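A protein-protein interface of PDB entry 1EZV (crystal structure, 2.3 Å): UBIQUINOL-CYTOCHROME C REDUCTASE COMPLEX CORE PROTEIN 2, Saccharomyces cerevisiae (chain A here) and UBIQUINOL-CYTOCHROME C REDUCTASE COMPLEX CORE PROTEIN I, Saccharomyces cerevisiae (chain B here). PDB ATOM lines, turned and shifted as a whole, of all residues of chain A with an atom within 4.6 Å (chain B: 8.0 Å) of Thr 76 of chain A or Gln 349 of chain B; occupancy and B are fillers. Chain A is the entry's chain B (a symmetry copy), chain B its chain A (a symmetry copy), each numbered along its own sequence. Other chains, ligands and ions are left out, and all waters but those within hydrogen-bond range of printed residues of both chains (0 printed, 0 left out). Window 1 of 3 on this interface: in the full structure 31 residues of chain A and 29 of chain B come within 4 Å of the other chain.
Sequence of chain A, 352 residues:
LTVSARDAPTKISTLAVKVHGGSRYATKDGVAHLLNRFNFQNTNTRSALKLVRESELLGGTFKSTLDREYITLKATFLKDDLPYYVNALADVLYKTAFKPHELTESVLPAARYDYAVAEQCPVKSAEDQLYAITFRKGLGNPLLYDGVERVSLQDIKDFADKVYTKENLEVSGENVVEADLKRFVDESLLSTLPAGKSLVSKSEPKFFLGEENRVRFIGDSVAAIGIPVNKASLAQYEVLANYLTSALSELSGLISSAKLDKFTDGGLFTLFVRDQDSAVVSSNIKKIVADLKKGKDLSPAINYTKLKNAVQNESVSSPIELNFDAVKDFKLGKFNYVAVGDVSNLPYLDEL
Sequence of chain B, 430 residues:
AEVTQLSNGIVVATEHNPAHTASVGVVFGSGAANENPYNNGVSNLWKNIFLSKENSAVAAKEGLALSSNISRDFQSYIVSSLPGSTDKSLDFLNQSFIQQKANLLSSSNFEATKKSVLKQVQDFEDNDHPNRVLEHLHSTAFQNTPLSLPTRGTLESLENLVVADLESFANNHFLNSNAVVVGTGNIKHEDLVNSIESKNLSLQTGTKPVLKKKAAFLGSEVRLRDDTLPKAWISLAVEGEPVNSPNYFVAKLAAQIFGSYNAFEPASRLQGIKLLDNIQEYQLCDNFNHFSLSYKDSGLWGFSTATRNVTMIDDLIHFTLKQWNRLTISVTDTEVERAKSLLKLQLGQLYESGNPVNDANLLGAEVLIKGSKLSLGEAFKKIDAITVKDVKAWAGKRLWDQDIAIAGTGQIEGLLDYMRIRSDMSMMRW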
ATOM      1  N   ILE A  12     -25.992 -10.991  -3.074  1.00  0.00           N
ATOM      2  CA  ILE A  12     -26.779 -10.198  -4.016  1.00  0.00           C
ATOM      3  C   ILE A  12     -28.057 -10.932  -4.399  1.00  0.00           C
ATOM      4  O   ILE A  12     -28.009 -11.998  -5.012  1.00  0.00           O
ATOM      5  CB  ILE A  12     -25.971  -9.891  -5.316  1.00  0.00           C
ATOM      6  CG1 ILE A  12     -24.696  -9.113  -4.980  1.00  0.00           C
ATOM      7  CG2 ILE A  12     -26.824  -9.105  -6.301  1.00  0.00           C
ATOM      8  CD1 ILE A  12     -24.941  -7.757  -4.352  1.00  0.00           C
ATOM      9  N   SER A  13     -29.199 -10.350  -4.047  1.00  0.00           N
ATOM     10  CA  SER A  13     -30.494 -10.879  -4.463  1.00  0.00           C
ATOM     11  C   SER A  13     -31.024 -10.075  -5.642  1.00  0.00           C
ATOM     12  O   SER A  13     -30.593  -8.946  -5.875  1.00  0.00           O
ATOM     13  CB  SER A  13     -31.492 -10.816  -3.303  1.00  0.00           C
ATOM     14  OG  SER A  13     -30.924 -11.317  -2.101  1.00  0.00           O
ATOM     15  N   THR A  14     -31.924 -10.672  -6.417  1.00  0.00           N
ATOM     16  CA  THR A  14     -32.551  -9.962  -7.523  1.00  0.00           C
ATOM     17  C   THR A  14     -34.032 -10.304  -7.669  1.00  0.00           C
ATOM     18  O   THR A  14     -34.396 -11.377  -8.149  1.00  0.00           O
ATOM     19  CB  THR A  14     -31.779 -10.184  -8.880  1.00  0.00           C
ATOM     20  OG1 THR A  14     -32.704 -10.453  -9.944  1.00  0.00           O
ATOM     21  CG2 THR A  14     -30.778 -11.329  -8.772  1.00  0.00           C
ATOM     22  N   GLY A  59     -28.117   0.338  -1.546  1.00  0.00           N
ATOM     23  CA  GLY A  59     -27.167  -0.429  -2.323  1.00  0.00           C
ATOM     24  C   GLY A  59     -27.887  -1.338  -3.288  1.00  0.00           C
ATOM     25  O   GLY A  59     -27.682  -2.548  -3.268  1.00  0.00           O
ATOM     26  N   GLY A  60     -28.757  -0.758  -4.108  1.00  0.00           N
ATOM     27  CA  GLY A  60     -29.465  -1.529  -5.112  1.00  0.00           C
ATOM     28  C   GLY A  60     -29.943  -0.661  -6.259  1.00  0.00           C
ATOM     29  O   GLY A  60     -30.128   0.543  -6.085  1.00  0.00           O
ATOM     30  N   THR A  61     -30.103  -1.257  -7.440  1.00  0.00           N
ATOM     31  CA  THR A  61     -30.577  -0.524  -8.611  1.00  0.00           C
ATOM     32  C   THR A  61     -31.842  -1.145  -9.190  1.00  0.00           C
ATOM     33  O   THR A  61     -32.184  -2.284  -8.883  1.00  0.00           O
ATOM     34  CB  THR A  61     -29.502  -0.456  -9.734  1.00  0.00           C
ATOM     35  OG1 THR A  61     -29.192  -1.777 -10.193  1.00  0.00           O
ATOM     36  CG2 THR A  61     -28.230   0.216  -9.226  1.00  0.00           C
ATOM     37  N   LYS A  74     -37.141  -5.436 -12.973  1.00  0.00           N
ATOM     38  CA  LYS A  74     -36.136  -6.146 -12.180  1.00  0.00           C
ATOM     39  C   LYS A  74     -35.474  -5.215 -11.165  1.00  0.00           C
ATOM     40  O   LYS A  74     -35.367  -4.014 -11.396  1.00  0.00           O
ATOM     41  CB  LYS A  74     -35.076  -6.739 -13.111  1.00  0.00           C
ATOM     42  CG  LYS A  74     -34.222  -7.836 -12.497  1.00  0.00           C
ATOM     43  CD  LYS A  74     -33.053  -8.179 -13.409  1.00  0.00           C
ATOM     44  CE  LYS A  74     -32.243  -9.347 -12.869  1.00  0.00           C
ATOM     45  NZ  LYS A  74     -30.946  -9.506 -13.592  1.00  0.00           N
ATOM     46  N   ALA A  75     -35.018  -5.781 -10.051  1.00  0.00           N
ATOM     47  CA  ALA A  75     -34.341  -5.010  -9.010  1.00  0.00           C
ATOM     48  C   ALA A  75     -33.212  -5.821  -8.393  1.00  0.00           C
ATOM     49  O   ALA A  75     -33.437  -6.893  -7.839  1.00  0.00           O
ATOM     50  CB  ALA A  75     -35.330  -4.594  -7.931  1.00  0.00           C
ATOM     51  N   THR A  76     -32.004  -5.276  -8.445  1.00  0.00           N
ATOM     52  CA  THR A  76     -30.819  -5.974  -7.968  1.00  0.00           C
ATOM     53  C   THR A  76     -30.292  -5.240  -6.743  1.00  0.00           C
ATOM     54  O   THR A  76     -30.154  -4.022  -6.767  1.00  0.00           O
ATOM     55  CB  THR A  76     -29.740  -5.994  -9.062  1.00  0.00           C
ATOM     56  OG1 THR A  76     -30.327  -6.418 -10.299  1.00  0.00           O
ATOM     57  CG2 THR A  76     -28.610  -6.930  -8.685  1.00  0.00           C
ATOM     58  N   PHE A  77     -30.006  -5.976  -5.673  1.00  0.00           N
ATOM     59  CA  PHE A  77     -29.739  -5.356  -4.377  1.00  0.00           C
ATOM     60  C   PHE A  77     -28.988  -6.269  -3.427  1.00  0.00           C
ATOM     61  O   PHE A  77     -28.793  -7.447  -3.712  1.00  0.00           O
ATOM     62  CB  PHE A  77     -31.053  -4.933  -3.720  1.00  0.00           C
ATOM     63  CG  PHE A  77     -32.084  -6.033  -3.655  1.00  0.00           C
ATOM     64  CD1 PHE A  77     -32.247  -6.785  -2.493  1.00  0.00           C
ATOM     65  CD2 PHE A  77     -32.905  -6.303  -4.747  1.00  0.00           C
ATOM     66  CE1 PHE A  77     -33.214  -7.790  -2.421  1.00  0.00           C
ATOM     67  CE2 PHE A  77     -33.872  -7.304  -4.682  1.00  0.00           C
ATOM     68  CZ  PHE A  77     -34.028  -8.048  -3.516  1.00  0.00           C
ATOM     69  N   LEU B 342     -22.778   1.237  -3.193  1.00  0.00           N
ATOM     70  CA  LEU B 342     -22.763   0.967  -4.625  1.00  0.00           C
ATOM     71  C   LEU B 342     -21.539   0.157  -5.052  1.00  0.00           C
ATOM     72  O   LEU B 342     -21.594  -0.581  -6.042  1.00  0.00           O
ATOM     73  CB  LEU B 342     -22.833   2.273  -5.409  1.00  0.00           C
ATOM     74  CG  LEU B 342     -24.146   3.043  -5.316  1.00  0.00           C
ATOM     75  CD1 LEU B 342     -23.970   4.396  -5.980  1.00  0.00           C
ATOM     76  CD2 LEU B 342     -25.269   2.261  -5.981  1.00  0.00           C
ATOM     77  N   LEU B 343     -20.444   0.296  -4.305  1.00  0.00           N
ATOM     78  CA  LEU B 343     -19.250  -0.516  -4.533  1.00  0.00           C
ATOM     79  C   LEU B 343     -19.535  -1.988  -4.195  1.00  0.00           C
ATOM     80  O   LEU B 343     -19.161  -2.891  -4.948  1.00  0.00           O
ATOM     81  CB  LEU B 343     -18.084  -0.006  -3.679  1.00  0.00           C
ATOM     82  CG  LEU B 343     -16.662  -0.028  -4.258  1.00  0.00           C
ATOM     83  CD1 LEU B 343     -15.662  -0.149  -3.123  1.00  0.00           C
ATOM     84  CD2 LEU B 343     -16.479  -1.167  -5.237  1.00  0.00           C
ATOM     85  N   LYS B 344     -20.250  -2.212  -3.093  1.00  0.00           N
ATOM     86  CA  LYS B 344     -20.657  -3.556  -2.688  1.00  0.00           C
ATOM     87  C   LYS B 344     -21.536  -4.190  -3.749  1.00  0.00           C
ATOM     88  O   LYS B 344     -21.327  -5.342  -4.134  1.00  0.00           O
ATOM     89  CB  LYS B 344     -21.427  -3.511  -1.372  1.00  0.00           C
ATOM     90  CG  LYS B 344     -20.581  -3.236  -0.145  1.00  0.00           C
ATOM     91  CD  LYS B 344     -21.467  -3.201   1.083  1.00  0.00           C
ATOM     92  CE  LYS B 344     -20.787  -2.505   2.241  1.00  0.00           C
ATOM     93  NZ  LYS B 344     -21.714  -2.396   3.399  1.00  0.00           N
ATOM     94  N   LEU B 345     -22.502  -3.420  -4.237  1.00  0.00           N
ATOM     95  CA  LEU B 345     -23.456  -3.916  -5.216  1.00  0.00           C
ATOM     96  C   LEU B 345     -22.764  -4.343  -6.501  1.00  0.00           C
ATOM     97  O   LEU B 345     -23.108  -5.369  -7.083  1.00  0.00           O
ATOM     98  CB  LEU B 345     -24.503  -2.847  -5.526  1.00  0.00           C
ATOM     99  CG  LEU B 345     -25.510  -3.180  -6.630  1.00  0.00           C
ATOM    100  CD1 LEU B 345     -26.459  -4.273  -6.158  1.00  0.00           C
ATOM    101  CD2 LEU B 345     -26.282  -1.930  -7.013  1.00  0.00           C
ATOM    102  N   GLN B 346     -21.780  -3.561  -6.934  1.00  0.00           N
ATOM    103  CA  GLN B 346     -21.120  -3.825  -8.207  1.00  0.00           C
ATOM    104  C   GLN B 346     -20.058  -4.904  -8.057  1.00  0.00           C
ATOM    105  O   GLN B 346     -19.863  -5.710  -8.960  1.00  0.00           O
ATOM    106  CB  GLN B 346     -20.505  -2.540  -8.784  1.00  0.00           C
ATOM    107  CG  GLN B 346     -19.163  -2.127  -8.178  1.00  0.00           C
ATOM    108  CD  GLN B 346     -18.089  -1.866  -9.229  1.00  0.00           C
ATOM    109  OE1 GLN B 346     -18.177  -2.353 -10.362  1.00  0.00           O
ATOM    110  NE2 GLN B 346     -17.061  -1.109  -8.852  1.00  0.00           N
ATOM    111  N   LEU B 347     -19.403  -4.934  -6.902  1.00  0.00           N
ATOM    112  CA  LEU B 347     -18.414  -5.962  -6.600  1.00  0.00           C
ATOM    113  C   LEU B 347     -19.099  -7.312  -6.427  1.00  0.00           C
ATOM    114  O   LEU B 347     -18.550  -8.353  -6.796  1.00  0.00           O
ATOM    115  CB  LEU B 347     -17.656  -5.600  -5.326  1.00  0.00           C
ATOM    116  CG  LEU B 347     -16.148  -5.837  -5.337  1.00  0.00           C
ATOM    117  CD1 LEU B 347     -15.532  -5.209  -6.578  1.00  0.00           C
ATOM    118  CD2 LEU B 347     -15.540  -5.253  -4.074  1.00  0.00           C
ATOM    119  N   GLY B 348     -20.301  -7.283  -5.853  1.00  0.00           N
ATOM    120  CA  GLY B 348     -21.140  -8.463  -5.802  1.00  0.00           C
ATOM    121  C   GLY B 348     -21.482  -8.968  -7.188  1.00  0.00           C
ATOM    122  O   GLY B 348     -21.125 -10.089  -7.536  1.00  0.00           O
ATOM    123  N   GLN B 349     -22.068  -8.104  -8.015  1.00  0.00           N
ATOM    124  CA  GLN B 349     -22.480  -8.477  -9.371  1.00  0.00           C
ATOM    125  C   GLN B 349     -21.334  -9.004 -10.241  1.00  0.00           C
ATOM    126  O   GLN B 349     -21.570  -9.630 -11.278  1.00  0.00           O
ATOM    127  CB  GLN B 349     -23.130  -7.282 -10.067  1.00  0.00           C
ATOM    128  CG  GLN B 349     -24.559  -7.013  -9.654  1.00  0.00           C
ATOM    129  CD  GLN B 349     -25.098  -5.734 -10.263  1.00  0.00           C
ATOM    130  OE1 GLN B 349     -24.683  -4.636  -9.893  1.00  0.00           O
ATOM    131  NE2 GLN B 349     -26.009  -5.870 -11.220  1.00  0.00           N
ATOM    132  N   LEU B 350     -20.099  -8.699  -9.845  1.00  0.00           N
ATOM    133  CA  LEU B 350     -18.915  -9.216 -10.526  1.00  0.00           C
ATOM    134  C   LEU B 350     -18.576 -10.619 -10.031  1.00  0.00           C
ATOM    135  O   LEU B 350     -18.545 -11.572 -10.811  1.00  0.00           O
ATOM    136  CB  LEU B 350     -17.711  -8.299 -10.282  1.00  0.00           C
ATOM    137  CG  LEU B 350     -17.149  -7.474 -11.444  1.00  0.00           C
ATOM    138  CD1 LEU B 350     -15.712  -7.089 -11.116  1.00  0.00           C
ATOM    139  CD2 LEU B 350     -17.204  -8.256 -12.750  1.00  0.00           C
ATOM    140  N   TYR B 351     -18.346 -10.730  -8.725  1.00  0.00           N
ATOM    141  CA  TYR B 351     -17.863 -11.960  -8.111  1.00  0.00           C
ATOM    142  C   TYR B 351     -18.886 -13.088  -8.137  1.00  0.00           C
ATOM    143  O   TYR B 351     -18.517 -14.264  -8.101  1.00  0.00           O
ATOM    144  CB  TYR B 351     -17.425 -11.691  -6.670  1.00  0.00           C
ATOM    145  CG  TYR B 351     -16.024 -11.131  -6.542  1.00  0.00           C
ATOM    146  CD1 TYR B 351     -15.201 -11.496  -5.475  1.00  0.00           C
ATOM    147  CD2 TYR B 351     -15.516 -10.237  -7.488  1.00  0.00           C
ATOM    148  CE1 TYR B 351     -13.908 -10.985  -5.351  1.00  0.00           C
ATOM    149  CE2 TYR B 351     -14.223  -9.722  -7.376  1.00  0.00           C
ATOM    150  CZ  TYR B 351     -13.425 -10.101  -6.307  1.00  0.00           C
ATOM    151  OH  TYR B 351     -12.144  -9.607  -6.198  1.00  0.00           O
ATOM    152  N   GLU B 352     -20.167 -12.736  -8.186  1.00  0.00           N
ATOM    153  CA  GLU B 352     -21.215 -13.744  -8.281  1.00  0.00           C
ATOM    154  C   GLU B 352     -22.213 -13.463  -9.394  1.00  0.00           C
ATOM    155  O   GLU B 352     -23.380 -13.155  -9.145  1.00  0.00           O
ATOM    156  CB  GLU B 352     -21.945 -13.919  -6.939  1.00  0.00           C
ATOM    157  CG  GLU B 352     -22.190 -12.642  -6.164  1.00  0.00           C
ATOM    158  CD  GLU B 352     -23.100 -12.849  -4.976  1.00  0.00           C
ATOM    159  OE1 GLU B 352     -24.328 -12.927  -5.185  1.00  0.00           O
ATOM    160  OE2 GLU B 352     -22.591 -12.922  -3.838  1.00  0.00           O
ATOM    161  N   SER B 353     -21.733 -13.567 -10.627  1.00  0.00           N
ATOM    162  CA  SER B 353     -22.612 -13.712 -11.777  1.00  0.00           C
ATOM    163  C   SER B 353     -23.020 -15.181 -11.892  1.00  0.00           C
ATOM    164  O   SER B 353     -22.477 -16.045 -11.190  1.00  0.00           O
ATOM    165  CB  SER B 353     -21.889 -13.278 -13.054  1.00  0.00           C
ATOM    166  OG  SER B 353     -22.785 -13.237 -14.152  1.00  0.00           O
ATOM    167  N   GLY B 354     -23.974 -15.462 -12.775  1.00  0.00           N
ATOM    168  CA  GLY B 354     -24.342 -16.841 -13.052  1.00  0.00           C
ATOM    169  C   GLY B 354     -23.521 -17.456 -14.173  1.00  0.00           C
ATOM    170  O   GLY B 354     -24.033 -18.264 -14.952  1.00  0.00           O
ATOM    171  N   ASN B 358     -16.431 -16.394 -15.915  1.00  0.00           N
ATOM    172  CA  ASN B 358     -16.032 -15.137 -15.283  1.00  0.00           C
ATOM    173  C   ASN B 358     -15.412 -15.442 -13.927  1.00  0.00           C
ATOM    174  O   ASN B 358     -14.380 -14.875 -13.564  1.00  0.00           O
ATOM    175  CB  ASN B 358     -17.237 -14.205 -15.092  1.00  0.00           C
ATOM    176  CG  ASN B 358     -17.900 -13.804 -16.407  1.00  0.00           C
ATOM    177  OD1 ASN B 358     -19.074 -13.435 -16.426  1.00  0.00           O
ATOM    178  ND2 ASN B 358     -17.147 -13.856 -17.504  1.00  0.00           N
ATOM    179  N   LEU B 362     -11.633 -14.472 -12.546  1.00  0.00           N
ATOM    180  CA  LEU B 362     -11.473 -13.695 -11.321  1.00  0.00           C
ATOM    181  C   LEU B 362     -10.689 -14.469 -10.261  1.00  0.00           C
ATOM    182  O   LEU B 362      -9.826 -13.905  -9.581  1.00  0.00           O
ATOM    183  CB  LEU B 362     -12.844 -13.290 -10.773  1.00  0.00           C
ATOM    184  CG  LEU B 362     -13.720 -12.455 -11.715  1.00  0.00           C
ATOM    185  CD1 LEU B 362     -15.073 -12.203 -11.067  1.00  0.00           C
ATOM    186  CD2 LEU B 362     -13.029 -11.137 -12.054  1.00  0.00           C
ATOM    187  N   LEU B 376     -15.744 -12.518  -0.807  1.00  0.00           N
ATOM    188  CA  LEU B 376     -16.619 -11.365  -0.994  1.00  0.00           C
ATOM    189  C   LEU B 376     -17.022 -10.719   0.331  1.00  0.00           C
ATOM    190  O   LEU B 376     -17.019  -9.494   0.452  1.00  0.00           O
ATOM    191  CB  LEU B 376     -17.869 -11.771  -1.771  1.00  0.00           C
ATOM    192  CG  LEU B 376     -18.687 -10.607  -2.326  1.00  0.00           C
ATOM    193  CD1 LEU B 376     -17.879  -9.880  -3.387  1.00  0.00           C
ATOM    194  CD2 LEU B 376     -19.992 -11.117  -2.908  1.00  0.00           C
ATOM    195  N   PHE B 380     -16.225  -6.715   1.847  1.00  0.00           N
ATOM    196  CA  PHE B 380     -17.240  -5.864   2.458  1.00  0.00           C
ATOM    197  C   PHE B 380     -16.821  -5.368   3.834  1.00  0.00           C
ATOM    198  O   PHE B 380     -17.193  -4.269   4.242  1.00  0.00           O
ATOM    199  CB  PHE B 380     -18.564  -6.619   2.579  1.00  0.00           C
ATOM    200  CG  PHE B 380     -19.292  -6.795   1.277  1.00  0.00           C
ATOM    201  CD1 PHE B 380     -18.602  -6.863   0.074  1.00  0.00           C
ATOM    202  CD2 PHE B 380     -20.670  -6.918   1.260  1.00  0.00           C
ATOM    203  CE1 PHE B 380     -19.277  -7.056  -1.131  1.00  0.00           C
ATOM    204  CE2 PHE B 380     -21.356  -7.111   0.060  1.00  0.00           C
ATOM    205  CZ  PHE B 380     -20.656  -7.183  -1.137  1.00  0.00           C
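Thr 76 of chain A touches just these residues of chain B: Leu 345 (3.8 Å) and Gln 349 (3.8 Å).
Gln 349 of chain B touches just one residue of chain A: Thr 76.
Of the printed residues of chain A, Leu 345 of chain B touches Gly 59, Gly 60, Thr 61, Thr 76 and Phe 77.
Of the printed residues of chain B, Phe 77 of chain A touches Leu 345 (3.9 Å).
Leu 342 of chain B touches none of the printed residues of chain A.
The nearest residue of chain B that does not touch Thr 76 of chain A is Gly 348 of chain B (7.6 Å).
The nearest printed residue of chain A that does not touch Gly 348 of chain B is Thr 76 of chain A (7.6 Å).
Gly 348 of chain B touches Ile 12 of chain A.
CD1 of Leu 345 of chain B touches O of Gly 59 of chain A, 3.6 Å away.
Leu 345 of chain B touches Gly 60 of chain A.
CG2 of Thr 61 of chain A touches CD2 of Leu 345 of chain B, at 3.6 Å.
O of Thr 76 of chain A touches CD1 of Leu 345 of chain B, at 3.8 Å.
Gln 349 of chain B touches Thr 76 of chain A.
CA of Phe 77 of chain A touches CD1 of Leu 345 of chain B (3.9 Å).
The backbone NH of Thr 61 of chain A is in hydrogen-bond range of the backbone carbonyl oxygen of Thr 76 of chain A (2.8 Å).
The backbone carbonyl oxygen of Leu 345 of chain B lies close to the side-chain amide oxygen of Gln 349 of chain B (3.3 Å).
O of Phe 77 of chain A lies within hydrogen-bond range of N of Ser 13 of chain A, at 3.0 Å.
Of the 17 printed residues of chain B, 4 touch a printed residue of chain A.
Hydrophobic or aromatic side chains of chain B within 4 Å of the printed part of chain A: Leu 345.
Of the 10 printed residues of chain A, 6 touch a printed residue of chain B.
Hydrophobic or aromatic side chains of chain A that line the printed part of chain B: Ile 12.
Among the printed residues, 8 pairs touch across the chains.
OE1 of Glu 352 of chain B sits at hydrogen-bond distance from N of Ile 12 of chain A (3.3 Å).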
